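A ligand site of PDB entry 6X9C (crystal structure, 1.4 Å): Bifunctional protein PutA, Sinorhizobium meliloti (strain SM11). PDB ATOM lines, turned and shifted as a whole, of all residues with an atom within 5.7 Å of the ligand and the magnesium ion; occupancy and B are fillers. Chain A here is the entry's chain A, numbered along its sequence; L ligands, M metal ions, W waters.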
ATOM      1  N   ILE A 705      -4.320  23.920  -4.955  1.00  0.00           N
ATOM      2  CA  ILE A 705      -3.050  24.630  -4.845  1.00  0.00           C
ATOM      3  C   ILE A 705      -2.028  23.630  -4.328  1.00  0.00           C
ATOM      4  O   ILE A 705      -2.257  22.978  -3.293  1.00  0.00           O
ATOM      5  CB  ILE A 705      -3.193  25.869  -3.937  1.00  0.00           C
ATOM      6  CG1 ILE A 705      -4.102  26.908  -4.614  1.00  0.00           C
ATOM      7  CG2 ILE A 705      -1.851  26.469  -3.640  1.00  0.00           C
ATOM      8  CD1 ILE A 705      -4.522  28.037  -3.706  1.00  0.00           C
ATOM      9  N   SER A 706      -0.932  23.478  -5.066  1.00  0.00           N
ATOM     10  CA  SER A 706       0.009  22.391  -4.836  1.00  0.00           C
ATOM     11  C   SER A 706       1.428  22.915  -4.697  1.00  0.00           C
ATOM     12  O   SER A 706       1.756  24.000  -5.198  1.00  0.00           O
ATOM     13  CB  SER A 706      -0.039  21.387  -6.000  1.00  0.00           C
ATOM     14  OG  SER A 706       0.225  22.033  -7.225  1.00  0.00           O
ATOM     15  N   PRO A 707       2.310  22.145  -4.045  1.00  0.00           N
ATOM     16  CA  PRO A 707       3.677  22.630  -3.773  1.00  0.00           C
ATOM     17  C   PRO A 707       4.690  22.103  -4.781  1.00  0.00           C
ATOM     18  O   PRO A 707       4.339  21.331  -5.683  1.00  0.00           O
ATOM     19  CB  PRO A 707       3.945  22.063  -2.383  1.00  0.00           C
ATOM     20  CG  PRO A 707       3.255  20.732  -2.426  1.00  0.00           C
ATOM     21  CD  PRO A 707       2.014  20.921  -3.301  1.00  0.00           C
ATOM     22  N   TRP A 708       5.946  22.517  -4.633  1.00  0.00           N
ATOM     23  CA  TRP A 708       7.007  22.194  -5.576  1.00  0.00           C
ATOM     24  C   TRP A 708       7.735  20.906  -5.228  1.00  0.00           C
ATOM     25  O   TRP A 708       8.517  20.406  -6.053  1.00  0.00           O
ATOM     26  CB  TRP A 708       8.026  23.338  -5.601  1.00  0.00           C
ATOM     27  CG  TRP A 708       8.338  23.784  -4.237  1.00  0.00           C
ATOM     28  CD1 TRP A 708       7.751  24.815  -3.552  1.00  0.00           C
ATOM     29  CD2 TRP A 708       9.252  23.172  -3.324  1.00  0.00           C
ATOM     30  NE1 TRP A 708       8.272  24.896  -2.285  1.00  0.00           N
ATOM     31  CE2 TRP A 708       9.193  23.895  -2.115  1.00  0.00           C
ATOM     32  CE3 TRP A 708      10.143  22.098  -3.426  1.00  0.00           C
ATOM     33  CZ2 TRP A 708       9.969  23.574  -1.002  1.00  0.00           C
ATOM     34  CZ3 TRP A 708      10.926  21.775  -2.320  1.00  0.00           C
ATOM     35  CH2 TRP A 708      10.827  22.513  -1.125  1.00  0.00           C
ATOM     36  N   ASN A 709       7.514  20.351  -4.034  1.00  0.00           N
ATOM     37  CA  ASN A 709       8.313  19.225  -3.573  1.00  0.00           C
ATOM     38  C   ASN A 709       7.790  17.880  -4.046  1.00  0.00           C
ATOM     39  O   ASN A 709       8.571  16.933  -4.152  1.00  0.00           O
ATOM     40  CB  ASN A 709       8.460  19.255  -2.049  1.00  0.00           C
ATOM     41  CG  ASN A 709       7.144  19.128  -1.330  1.00  0.00           C
ATOM     42  OD1 ASN A 709       6.086  19.457  -1.866  1.00  0.00           O
ATOM     43  ND2 ASN A 709       7.198  18.660  -0.088  1.00  0.00           N
ATOM     44  N   ILE A 714       1.431  15.037  -5.615  1.00  0.00           N
ATOM     45  CA  ILE A 714       0.425  15.742  -4.827  1.00  0.00           C
ATOM     46  C   ILE A 714      -0.446  16.604  -5.737  1.00  0.00           C
ATOM     47  O   ILE A 714      -1.662  16.727  -5.525  1.00  0.00           O
ATOM     48  CB  ILE A 714       1.092  16.544  -3.694  1.00  0.00           C
ATOM     49  CG1 ILE A 714       1.475  15.590  -2.565  1.00  0.00           C
ATOM     50  CG2 ILE A 714       0.161  17.670  -3.179  1.00  0.00           C
ATOM     51  CD1 ILE A 714       2.389  16.229  -1.570  1.00  0.00           C
ATOM     52  N   LYS A 732      -3.629  25.272  -9.596  1.00  0.00           N
ATOM     53  CA  LYS A 732      -2.611  26.313  -9.462  1.00  0.00           C
ATOM     54  C   LYS A 732      -1.334  25.665  -8.930  1.00  0.00           C
ATOM     55  O   LYS A 732      -1.211  25.439  -7.713  1.00  0.00           O
ATOM     56  CB  LYS A 732      -3.095  27.412  -8.506  1.00  0.00           C
ATOM     57  CG  LYS A 732      -2.621  28.820  -8.859  1.00  0.00           C
ATOM     58  CD  LYS A 732      -1.097  28.945  -8.847  1.00  0.00           C
ATOM     59  CE  LYS A 732      -0.543  28.793  -7.432  1.00  0.00           C
ATOM     60  NZ  LYS A 732       0.947  28.911  -7.448  1.00  0.00           N
ATOM     61  N   PRO A 733      -0.392  25.309  -9.790  1.00  0.00           N
ATOM     62  CA  PRO A 733       0.824  24.643  -9.322  1.00  0.00           C
ATOM     63  C   PRO A 733       1.798  25.640  -8.738  1.00  0.00           C
ATOM     64  O   PRO A 733       1.740  26.841  -9.004  1.00  0.00           O
ATOM     65  CB  PRO A 733       1.398  24.038 -10.606  1.00  0.00           C
ATOM     66  CG  PRO A 733       0.991  25.009 -11.677  1.00  0.00           C
ATOM     67  CD  PRO A 733      -0.409  25.462 -11.264  1.00  0.00           C
ATOM     68  N   ALA A 734       2.711  25.108  -7.921  1.00  0.00           N
ATOM     69  CA  ALA A 734       3.797  25.925  -7.384  1.00  0.00           C
ATOM     70  C   ALA A 734       4.519  26.660  -8.503  1.00  0.00           C
ATOM     71  O   ALA A 734       4.738  26.117  -9.590  1.00  0.00           O
ATOM     72  CB  ALA A 734       4.805  25.007  -6.666  1.00  0.00           C
ATOM     73  N   GLU A 735       4.897  27.907  -8.233  1.00  0.00           N
ATOM     74  CA  GLU A 735       5.546  28.709  -9.258  1.00  0.00           C
ATOM     75  C   GLU A 735       6.883  28.131  -9.692  1.00  0.00           C
ATOM     76  O   GLU A 735       7.315  28.366 -10.825  1.00  0.00           O
ATOM     77  CB  GLU A 735       5.695  30.165  -8.806  1.00  0.00           C
ATOM     78  CG  GLU A 735       6.435  30.363  -7.482  1.00  0.00           C
ATOM     79  CD  GLU A 735       5.509  30.421  -6.272  1.00  0.00           C
ATOM     80  OE1 GLU A 735       4.455  29.741  -6.272  1.00  0.00           O
ATOM     81  OE2 GLU A 735       5.839  31.133  -5.301  1.00  0.00           O
ATOM     82  N   GLU A 736       7.519  27.328  -8.838  1.00  0.00           N
ATOM     83  CA  GLU A 736       8.807  26.722  -9.181  1.00  0.00           C
ATOM     84  C   GLU A 736       8.673  25.527 -10.126  1.00  0.00           C
ATOM     85  O   GLU A 736       9.644  25.185 -10.809  1.00  0.00           O
ATOM     86  CB  GLU A 736       9.529  26.256  -7.918  1.00  0.00           C
ATOM     87  CG  GLU A 736       9.874  27.369  -6.946  1.00  0.00           C
ATOM     88  CD  GLU A 736       8.767  27.686  -5.947  1.00  0.00           C
ATOM     89  OE1 GLU A 736       9.032  28.489  -5.023  1.00  0.00           O
ATOM     90  OE2 GLU A 736       7.650  27.143  -6.077  1.00  0.00           O
ATOM     91  N   GLY A 763       1.454  30.274 -11.942  1.00  0.00           N
ATOM     92  CA  GLY A 763       1.781  31.560 -11.353  1.00  0.00           C
ATOM     93  C   GLY A 763       2.124  31.411  -9.883  1.00  0.00           C
ATOM     94  O   GLY A 763       2.222  30.313  -9.358  1.00  0.00           O
ATOM     95  N   ASP A 764       2.287  32.565  -9.251  1.00  0.00           N
ATOM     96  CA  ASP A 764       2.761  32.639  -7.871  1.00  0.00           C
ATOM     97  C   ASP A 764       1.569  32.678  -6.905  1.00  0.00           C
ATOM     98  O   ASP A 764       0.440  32.321  -7.261  1.00  0.00           O
ATOM     99  CB  ASP A 764       3.732  33.814  -7.711  1.00  0.00           C
ATOM    100  CG  ASP A 764       3.095  35.164  -8.049  1.00  0.00           C
ATOM    101  OD1 ASP A 764       1.857  35.290  -7.971  1.00  0.00           O
ATOM    102  OD2 ASP A 764       3.848  36.091  -8.396  1.00  0.00           O
ATOM    103  N   GLY A 765       1.806  33.126  -5.668  1.00  0.00           N
ATOM    104  CA  GLY A 765       0.754  33.133  -4.673  1.00  0.00           C
ATOM    105  C   GLY A 765      -0.390  34.066  -5.017  1.00  0.00           C
ATOM    106  O   GLY A 765      -1.530  33.850  -4.569  1.00  0.00           O
ATOM    107  N   ARG A 766      -0.124  35.111  -5.804  1.00  0.00           N
ATOM    108  CA  ARG A 766      -1.191  36.027  -6.197  1.00  0.00           C
ATOM    109  C   ARG A 766      -2.245  35.318  -7.033  1.00  0.00           C
ATOM    110  O   ARG A 766      -3.444  35.588  -6.907  1.00  0.00           O
ATOM    111  CB  ARG A 766      -0.612  37.219  -6.960  1.00  0.00           C
ATOM    112  N   GLY A 768      -2.843  32.022  -6.788  1.00  0.00           N
ATOM    113  CA  GLY A 768      -3.545  31.220  -5.784  1.00  0.00           C
ATOM    114  C   GLY A 768      -4.565  32.028  -5.014  1.00  0.00           C
ATOM    115  O   GLY A 768      -5.695  31.583  -4.822  1.00  0.00           O
ATOM    116  N   ALA A 769      -4.192  33.239  -4.597  1.00  0.00           N
ATOM    117  CA  ALA A 769      -5.100  34.044  -3.776  1.00  0.00           C
ATOM    118  C   ALA A 769      -6.319  34.489  -4.585  1.00  0.00           C
ATOM    119  O   ALA A 769      -7.441  34.479  -4.072  1.00  0.00           O
ATOM    120  CB  ALA A 769      -4.354  35.258  -3.206  1.00  0.00           C
ATOM    121  N   VAL A 772      -8.667  31.568  -4.738  1.00  0.00           N
ATOM    122  CA  VAL A 772      -9.328  31.307  -3.459  1.00  0.00           C
ATOM    123  C   VAL A 772     -10.459  32.307  -3.220  1.00  0.00           C
ATOM    124  O   VAL A 772     -11.550  31.924  -2.800  1.00  0.00           O
ATOM    125  CB  VAL A 772      -8.291  31.314  -2.317  1.00  0.00           C
ATOM    126  CG1 VAL A 772      -8.984  31.287  -0.959  1.00  0.00           C
ATOM    127  CG2 VAL A 772      -7.346  30.123  -2.444  1.00  0.00           C
ATOM    128  N   PHE A 782      -5.265  22.319  -0.517  1.00  0.00           N
ATOM    129  CA  PHE A 782      -4.002  23.031  -0.372  1.00  0.00           C
ATOM    130  C   PHE A 782      -2.970  22.118   0.269  1.00  0.00           C
ATOM    131  O   PHE A 782      -3.251  21.487   1.290  1.00  0.00           O
ATOM    132  CB  PHE A 782      -4.178  24.284   0.502  1.00  0.00           C
ATOM    133  CG  PHE A 782      -2.883  24.977   0.795  1.00  0.00           C
ATOM    134  CD1 PHE A 782      -2.337  25.866  -0.115  1.00  0.00           C
ATOM    135  CD2 PHE A 782      -2.190  24.718   1.967  1.00  0.00           C
ATOM    136  CE1 PHE A 782      -1.129  26.509   0.126  1.00  0.00           C
ATOM    137  CE2 PHE A 782      -0.969  25.355   2.222  1.00  0.00           C
ATOM    138  CZ  PHE A 782      -0.446  26.243   1.305  1.00  0.00           C
ATOM    139  N   THR A 783      -1.789  22.067  -0.323  1.00  0.00           N
ATOM    140  CA  THR A 783      -0.643  21.432   0.323  1.00  0.00           C
ATOM    141  C   THR A 783       0.512  22.418   0.265  1.00  0.00           C
ATOM    142  O   THR A 783       0.867  22.906  -0.825  1.00  0.00           O
ATOM    143  CB  THR A 783      -0.280  20.110  -0.353  1.00  0.00           C
ATOM    144  OG1 THR A 783      -1.428  19.241  -0.340  1.00  0.00           O
ATOM    145  CG2 THR A 783       0.861  19.441   0.397  1.00  0.00           C
ATOM    146  N   GLY A 784       1.093  22.716   1.421  1.00  0.00           N
ATOM    147  CA  GLY A 784       2.128  23.742   1.505  1.00  0.00           C
ATOM    148  C   GLY A 784       2.310  24.181   2.945  1.00  0.00           C
ATOM    149  O   GLY A 784       2.156  23.388   3.869  1.00  0.00           O
ATOM    150  N   SER A 785       2.660  25.455   3.110  1.00  0.00           N
ATOM    151  CA  SER A 785       3.022  25.969   4.427  1.00  0.00           C
ATOM    152  C   SER A 785       1.805  26.183   5.315  1.00  0.00           C
ATOM    153  O   SER A 785       0.678  26.407   4.846  1.00  0.00           O
ATOM    154  CB  SER A 785       3.766  27.287   4.300  1.00  0.00           C
ATOM    155  OG  SER A 785       2.946  28.337   3.815  1.00  0.00           O
ATOM    156  N   THR A 786       2.043  26.155   6.633  1.00  0.00           N
ATOM    157  CA  THR A 786       0.993  26.485   7.583  1.00  0.00           C
ATOM    158  C   THR A 786       0.560  27.930   7.449  1.00  0.00           C
ATOM    159  O   THR A 786      -0.631  28.240   7.570  1.00  0.00           O
ATOM    160  CB  THR A 786       1.478  26.251   9.016  1.00  0.00           C
ATOM    161  OG1 THR A 786       2.662  27.032   9.248  1.00  0.00           O
ATOM    162  CG2 THR A 786       1.774  24.801   9.247  1.00  0.00           C
ATOM    163  N   GLU A 787       1.521  28.847   7.231  1.00  0.00           N
ATOM    164  CA  GLU A 787       1.190  30.262   7.161  1.00  0.00           C
ATOM    165  C   GLU A 787       0.240  30.543   6.009  1.00  0.00           C
ATOM    166  O   GLU A 787      -0.726  31.302   6.155  1.00  0.00           O
ATOM    167  CB  GLU A 787       2.463  31.100   6.992  1.00  0.00           C
ATOM    168  CG  GLU A 787       3.460  30.963   8.115  1.00  0.00           C
ATOM    169  CD  GLU A 787       4.506  29.899   7.859  1.00  0.00           C
ATOM    170  OE1 GLU A 787       4.204  28.896   7.188  1.00  0.00           O
ATOM    171  OE2 GLU A 787       5.654  30.085   8.330  1.00  0.00           O
ATOM    172  N   VAL A 788       0.502  29.934   4.856  1.00  0.00           N
ATOM    173  CA  VAL A 788      -0.369  30.164   3.710  1.00  0.00           C
ATOM    174  C   VAL A 788      -1.725  29.484   3.905  1.00  0.00           C
ATOM    175  O   VAL A 788      -2.762  30.064   3.577  1.00  0.00           O
ATOM    176  CB  VAL A 788       0.349  29.783   2.394  1.00  0.00           C
ATOM    177  CG1 VAL A 788      -0.644  29.791   1.259  1.00  0.00           C
ATOM    178  CG2 VAL A 788       1.457  30.786   2.102  1.00  0.00           C
ATOM    179  N   LEU A 791      -3.678  31.838   5.928  1.00  0.00           N
ATOM    180  CA  LEU A 791      -4.181  32.952   5.130  1.00  0.00           C
ATOM    181  C   LEU A 791      -5.361  32.527   4.267  1.00  0.00           C
ATOM    182  O   LEU A 791      -6.341  33.272   4.123  1.00  0.00           O
ATOM    183  CB  LEU A 791      -3.062  33.535   4.278  1.00  0.00           C
ATOM    184  CG  LEU A 791      -1.979  34.322   5.032  1.00  0.00           C
ATOM    185  CD1 LEU A 791      -0.819  34.614   4.099  1.00  0.00           C
ATOM    186  CD2 LEU A 791      -2.558  35.612   5.599  1.00  0.00           C
ATOM    187  N   ILE A 792      -5.292  31.325   3.685  1.00  0.00           N
ATOM    188  CA  ILE A 792      -6.418  30.823   2.898  1.00  0.00           C
ATOM    189  C   ILE A 792      -7.654  30.648   3.778  1.00  0.00           C
ATOM    190  O   ILE A 792      -8.768  31.025   3.400  1.00  0.00           O
ATOM    191  CB  ILE A 792      -6.037  29.530   2.160  1.00  0.00           C
ATOM    192  CG1 ILE A 792      -5.042  29.850   1.049  1.00  0.00           C
ATOM    193  CG2 ILE A 792      -7.290  28.831   1.612  1.00  0.00           C
ATOM    194  CD1 ILE A 792      -4.414  28.629   0.422  1.00  0.00           C
ATOM    195  N   GLU A 812      -2.836  20.042   3.929  1.00  0.00           N
ATOM    196  CA  GLU A 812      -1.732  19.337   4.571  1.00  0.00           C
ATOM    197  C   GLU A 812      -0.562  20.301   4.661  1.00  0.00           C
ATOM    198  O   GLU A 812      -0.182  20.894   3.647  1.00  0.00           O
ATOM    199  CB  GLU A 812      -1.307  18.081   3.806  1.00  0.00           C
ATOM    200  CG  GLU A 812      -0.158  17.314   4.525  1.00  0.00           C
ATOM    201  CD  GLU A 812       1.177  17.391   3.812  1.00  0.00           C
ATOM    202  OE1 GLU A 812       1.346  16.694   2.782  1.00  0.00           O
ATOM    203  OE2 GLU A 812       2.062  18.137   4.266  1.00  0.00           O
ATOM    204  N   THR A 813       0.018  20.437   5.854  1.00  0.00           N
ATOM    205  CA  THR A 813       0.950  21.528   6.102  1.00  0.00           C
ATOM    206  C   THR A 813       2.223  21.109   6.827  1.00  0.00           C
ATOM    207  O   THR A 813       2.776  21.894   7.605  1.00  0.00           O
ATOM    208  CB  THR A 813       0.261  22.671   6.839  1.00  0.00           C
ATOM    209  OG1 THR A 813      -0.406  22.139   7.987  1.00  0.00           O
ATOM    210  CG2 THR A 813      -0.748  23.350   5.942  1.00  0.00           C
ATOM    211  N   GLY A 814       2.723  19.922   6.575  1.00  0.00           N
ATOM    212  CA  GLY A 814       4.072  19.623   7.051  1.00  0.00           C
ATOM    213  C   GLY A 814       4.101  19.145   8.498  1.00  0.00           C
ATOM    214  O   GLY A 814       3.064  18.841   9.100  1.00  0.00           O
ATOM    215  N   GLN A 844      13.273  17.680   1.753  1.00  0.00           N
ATOM    216  CA  GLN A 844      12.146  18.481   1.312  1.00  0.00           C
ATOM    217  C   GLN A 844      10.850  17.683   1.234  1.00  0.00           C
ATOM    218  O   GLN A 844       9.959  18.055   0.475  1.00  0.00           O
ATOM    219  CB  GLN A 844      12.472  19.172  -0.011  1.00  0.00           C
ATOM    220  CG  GLN A 844      13.635  20.137   0.115  1.00  0.00           C
ATOM    221  CD  GLN A 844      13.996  20.783  -1.216  1.00  0.00           C
ATOM    222  OE1 GLN A 844      14.170  21.994  -1.297  1.00  0.00           O
ATOM    223  NE2 GLN A 844      14.122  19.974  -2.250  1.00  0.00           N
ATOM    224  N   ARG A 845      10.737  16.603   1.992  1.00  0.00           N
ATOM    225  CA  ARG A 845       9.468  15.912   2.159  1.00  0.00           C
ATOM    226  C   ARG A 845       8.807  16.445   3.411  1.00  0.00           C
ATOM    227  O   ARG A 845       9.471  16.686   4.424  1.00  0.00           O
ATOM    228  CB  ARG A 845       9.699  14.413   2.360  1.00  0.00           C
ATOM    229  CG  ARG A 845      10.264  13.668   1.170  1.00  0.00           C
ATOM    230  CD  ARG A 845      10.388  12.203   1.526  1.00  0.00           C
ATOM    231  NE  ARG A 845      11.040  11.463   0.457  1.00  0.00           N
ATOM    232  CZ  ARG A 845      10.403  10.658  -0.379  1.00  0.00           C
ATOM    233  NH1 ARG A 845       9.068  10.488  -0.271  1.00  0.00           N
ATOM    234  NH2 ARG A 845      11.076  10.012  -1.330  1.00  0.00           N
ATOM    235  N   CYS A 846       7.484  16.609   3.355  1.00  0.00           N
ATOM    236  CA  CYS A 846       6.765  16.973   4.565  1.00  0.00           C
ATOM    237  C   CYS A 846       6.953  15.925   5.652  1.00  0.00           C
ATOM    238  O   CYS A 846       6.868  16.261   6.846  1.00  0.00           O
ATOM    239  CB  CYS A 846       5.275  17.136   4.266  1.00  0.00           C
ATOM    240  SG  CYS A 846       4.502  15.612   3.713  1.00  0.00           S
ATOM    241  N   GLU A 942       9.471  24.356  11.668  1.00  0.00           N
ATOM    242  CA  GLU A 942       9.835  23.359  10.665  1.00  0.00           C
ATOM    243  C   GLU A 942      10.908  23.940   9.756  1.00  0.00           C
ATOM    244  O   GLU A 942      10.736  25.026   9.179  1.00  0.00           O
ATOM    245  CB  GLU A 942       8.619  22.979   9.825  1.00  0.00           C
ATOM    246  CG  GLU A 942       8.932  22.029   8.660  1.00  0.00           C
ATOM    247  CD  GLU A 942       7.759  21.842   7.701  1.00  0.00           C
ATOM    248  OE1 GLU A 942       7.292  20.698   7.540  1.00  0.00           O
ATOM    249  OE2 GLU A 942       7.306  22.842   7.111  1.00  0.00           O
ATOM    250  N   PHE A 944      12.809  23.191   6.441  1.00  0.00           N
ATOM    251  CA  PHE A 944      12.427  22.322   5.329  1.00  0.00           C
ATOM    252  C   PHE A 944      13.628  22.050   4.432  1.00  0.00           C
ATOM    253  O   PHE A 944      13.722  22.490   3.282  1.00  0.00           O
ATOM    254  CB  PHE A 944      11.296  22.978   4.551  1.00  0.00           C
ATOM    255  CG  PHE A 944      10.380  21.994   3.903  1.00  0.00           C
ATOM    256  CD1 PHE A 944       9.554  21.206   4.687  1.00  0.00           C
ATOM    257  CD2 PHE A 944      10.316  21.862   2.518  1.00  0.00           C
ATOM    258  CE1 PHE A 944       8.696  20.293   4.113  1.00  0.00           C
ATOM    259  CE2 PHE A 944       9.451  20.952   1.938  1.00  0.00           C
ATOM    260  CZ  PHE A 944       8.657  20.150   2.742  1.00  0.00           C
HETATM  261  P1  LIG L   1       3.945  28.085   0.157  1.00  0.00           P
HETATM  262  O1  LIG L   1       3.007  27.262   1.001  1.00  0.00           O
HETATM  263  O2  LIG L   1       4.089  29.574   0.143  1.00  0.00           O
HETATM  264  O3  LIG L   1       3.436  27.703  -1.455  1.00  0.00           O
HETATM  265  C1  LIG L   1       2.585  26.623  -1.419  1.00  0.00           C
HETATM  266  C2  LIG L   1       1.514  26.864  -2.545  1.00  0.00           C
HETATM  267  O4  LIG L   1       0.686  27.923  -2.110  1.00  0.00           O
HETATM  268  C3  LIG L   1       2.174  27.343  -3.893  1.00  0.00           C
HETATM  269  O5  LIG L   1       1.375  26.867  -4.959  1.00  0.00           O
HETATM  270  C4  LIG L   1       2.071  28.856  -3.795  1.00  0.00           C
HETATM  271  O6  LIG L   1       1.994  29.462  -5.047  1.00  0.00           O
HETATM  272  C5  LIG L   1       0.690  28.958  -3.097  1.00  0.00           C
HETATM  273  N1  LIG L   1       0.508  30.176  -2.374  1.00  0.00           N
HETATM  274  C6  LIG L   1       1.473  30.992  -1.739  1.00  0.00           C
HETATM  275  N2  LIG L   1       0.910  32.050  -1.139  1.00  0.00           N
HETATM  276  C7  LIG L   1      -0.458  31.918  -1.384  1.00  0.00           C
HETATM  277  C8  LIG L   1      -1.569  32.711  -1.004  1.00  0.00           C
HETATM  278  N3  LIG L   1      -1.421  33.846  -0.266  1.00  0.00           N
HETATM  279  N4  LIG L   1      -2.828  32.351  -1.383  1.00  0.00           N
HETATM  280  C9  LIG L   1      -2.934  31.210  -2.106  1.00  0.00           C
HETATM  281  N5  LIG L   1      -1.974  30.359  -2.539  1.00  0.00           N
HETATM  282  C10 LIG L   1      -0.737  30.759  -2.137  1.00  0.00           C
HETATM  283  O7  LIG L   1       5.279  27.215   0.349  1.00  0.00           O
HETATM  284  P2  LIG L   1       6.697  27.941   0.001  1.00  0.00           P
HETATM  285  O8  LIG L   1       6.913  29.376   0.368  1.00  0.00           O
HETATM  286  O9  LIG L   1       7.069  27.285  -1.301  1.00  0.00           O
HETATM  287  O10 LIG L   1       7.761  27.106   1.056  1.00  0.00           O
HETATM  288  C11 LIG L   1       7.642  27.733   2.281  1.00  0.00           C
HETATM  289  C12 LIG L   1       7.580  26.683   3.387  1.00  0.00           C
HETATM  290  O11 LIG L   1       6.311  26.034   3.329  1.00  0.00           O
HETATM  291  C13 LIG L   1       8.608  25.552   3.121  1.00  0.00           C
HETATM  292  O12 LIG L   1       9.864  25.942   3.587  1.00  0.00           O
HETATM  293  C14 LIG L   1       7.979  24.449   3.994  1.00  0.00           C
HETATM  294  O13 LIG L   1       8.205  24.627   5.375  1.00  0.00           O
HETATM  295  C15 LIG L   1       6.450  24.668   3.739  1.00  0.00           C
HETATM  296  N6  LIG L   1       5.965  23.806   2.641  1.00  0.00           N
HETATM  297  C16 LIG L   1       5.289  22.628   2.916  1.00  0.00           C
HETATM  298  C17 LIG L   1       5.053  21.742   1.904  1.00  0.00           C
HETATM  299  C18 LIG L   1       4.458  20.456   2.232  1.00  0.00           C
HETATM  300  O14 LIG L   1       4.694  19.396   1.607  1.00  0.00           O
HETATM  301  N7  LIG L   1       3.568  20.432   3.262  1.00  0.00           N
HETATM  302  C19 LIG L   1       5.725  21.894   0.571  1.00  0.00           C
HETATM  303  C20 LIG L   1       6.046  23.293   0.301  1.00  0.00           C
HETATM  304  C21 LIG L   1       6.195  24.170   1.291  1.00  0.00           C
HETATM  305 MG    MG M   1       5.579  30.954  -0.880  1.00  0.00          MG
HETATM  306  O   HOH W   1       5.632  27.622  -4.225  1.00  0.00           O
HETATM  307  O   HOH W   2       3.437  17.336   1.107  1.00  0.00           O
HETATM  308  O   HOH W   3      10.510  27.368  -0.331  1.00  0.00           O
HETATM  309  O   HOH W   4      11.703  25.571   1.545  1.00  0.00           O
HETATM  310  O   HOH W   5      -5.119  33.491  -0.053  1.00  0.00           O
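OE2 of Glu 942 lies within hydrogen-bond range of O13 of the ligand (2.6 Å). An oxygen (O6) of the ligand is in hydrogen-bond range of the side-chain amino group (NZ) of Lys 732 (2.7 Å). O6 of the ligand is in hydrogen-bond range of OE1 of Glu 735, at 2.8 Å. N of Ser 785 sits at hydrogen-bond distance from O1 of the ligand. The side-chain hydroxyl (OG) of Ser 785 sits at hydrogen-bond distance from an oxygen (O1) of the ligand (3.0 Å). The indole nitrogen (NE1) of Trp 708 sits at hydrogen-bond distance from an oxygen (O9) of the ligand. O of Ser 706 is in hydrogen-bond range of O5 of the ligand (2.9 Å). N7 of the ligand is in hydrogen-bond range of OE2 of Glu 812 (2.9 Å). An oxygen (O14) of the ligand lies within hydrogen-bond range of the side-chain amide nitrogen of Asn 709 (3.1 Å). O of Gly 784 is in hydrogen-bond range of N7 of the ligand (3.3 Å).
NZ of Lys 732 is in salt-bridge range of OE1 of Glu 735 (3.8 Å). The side-chain amino group of Lys 732 lies within hydrogen-bond range of the backbone carbonyl oxygen of Asp 764. O of Gly 763 is in hydrogen-bond range of NZ of Lys 732 (2.7 Å). OG of Ser 785 lies within hydrogen-bond range of N of Val 788 (3.1 Å). The backbone NH of Ala 734 sits at hydrogen-bond distance from the backbone carbonyl oxygen of Ser 706. The backbone NH (N) of Glu 812 sits at hydrogen-bond distance from the backbone carbonyl oxygen (O) of Phe 782, at 3.0 Å. The side-chain carboxylate (OE2) of Glu 812 is in hydrogen-bond range of the backbone NH (N) of Gly 814 (3.0 Å). N of Arg 766 sits at hydrogen-bond distance from OD1 of Asp 764.
The backbone NH (N) of Gly 814 sits close to a nitrogen (N7) of the ligand, 3.5 Å away. Ile 705 touches the ligand. CB of Pro 707 touches C19 of the ligand, 3.5 Å away. C of Pro 733 touches O5 of the ligand, at 3.996 Å. Ala 734 touches the ligand. C of Asp 764 touches O6 of the ligand, 3.7 Å away. Gly 765 touches the ligand. C of Gly 768 touches C9 of the ligand, at 3.4 Å. Ala 769 touches the ligand (N to C9, 3.5 Å). CE1 of Phe 782 touches O4 of the ligand, 3.2 Å away. Val 788 touches the ligand (CG1 to C7, 3.4 Å). CD1 of Ile 792 touches C9 of the ligand, 3.9 Å away. C of Thr 813 touches N7 of the ligand, at 3.9 Å. Cys 846 touches the ligand (CB to O14, 3.5 Å). Phe 944 touches the ligand. Hydrophobic or aromatic side chains within 4 Å of the ligand: Ile 705, Pro 707, Trp 708, Ala 769, Phe 782, Val 788, Ile 792 and Phe 944. Within 4 Å of the ligand: Ile 705, Ser 706, Pro 707, Trp 708, Asn 709, Lys 732, Pro 733, Ala 734, Glu 735, Asp 764, Gly 765, Gly 768, Ala 769, Phe 782, Gly 784, Ser 785, Val 788, Ile 792, Glu 812, Thr 813, Gly 814, Cys 846, Glu 942 and Phe 944.
No residue comes within 4 Å of the magnesium ion.
The magnesium ion is bound by O2 of the ligand (2.3 Å) and O8 of the ligand (2.4 Å). The magnesium ion has two donor atoms within binding distance.
Water W2 lies within hydrogen-bond range of O14 of the ligand (2.5 Å), OE1 of Glu 812 (2.8 Å) and SG of Cys 846 (3.3 Å). Water W1 lies within hydrogen-bond range of OE2 of Glu 736 (2.8 Å), OE1 of Glu 735 (3.2 Å) and O9 of the ligand (3.3 Å).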
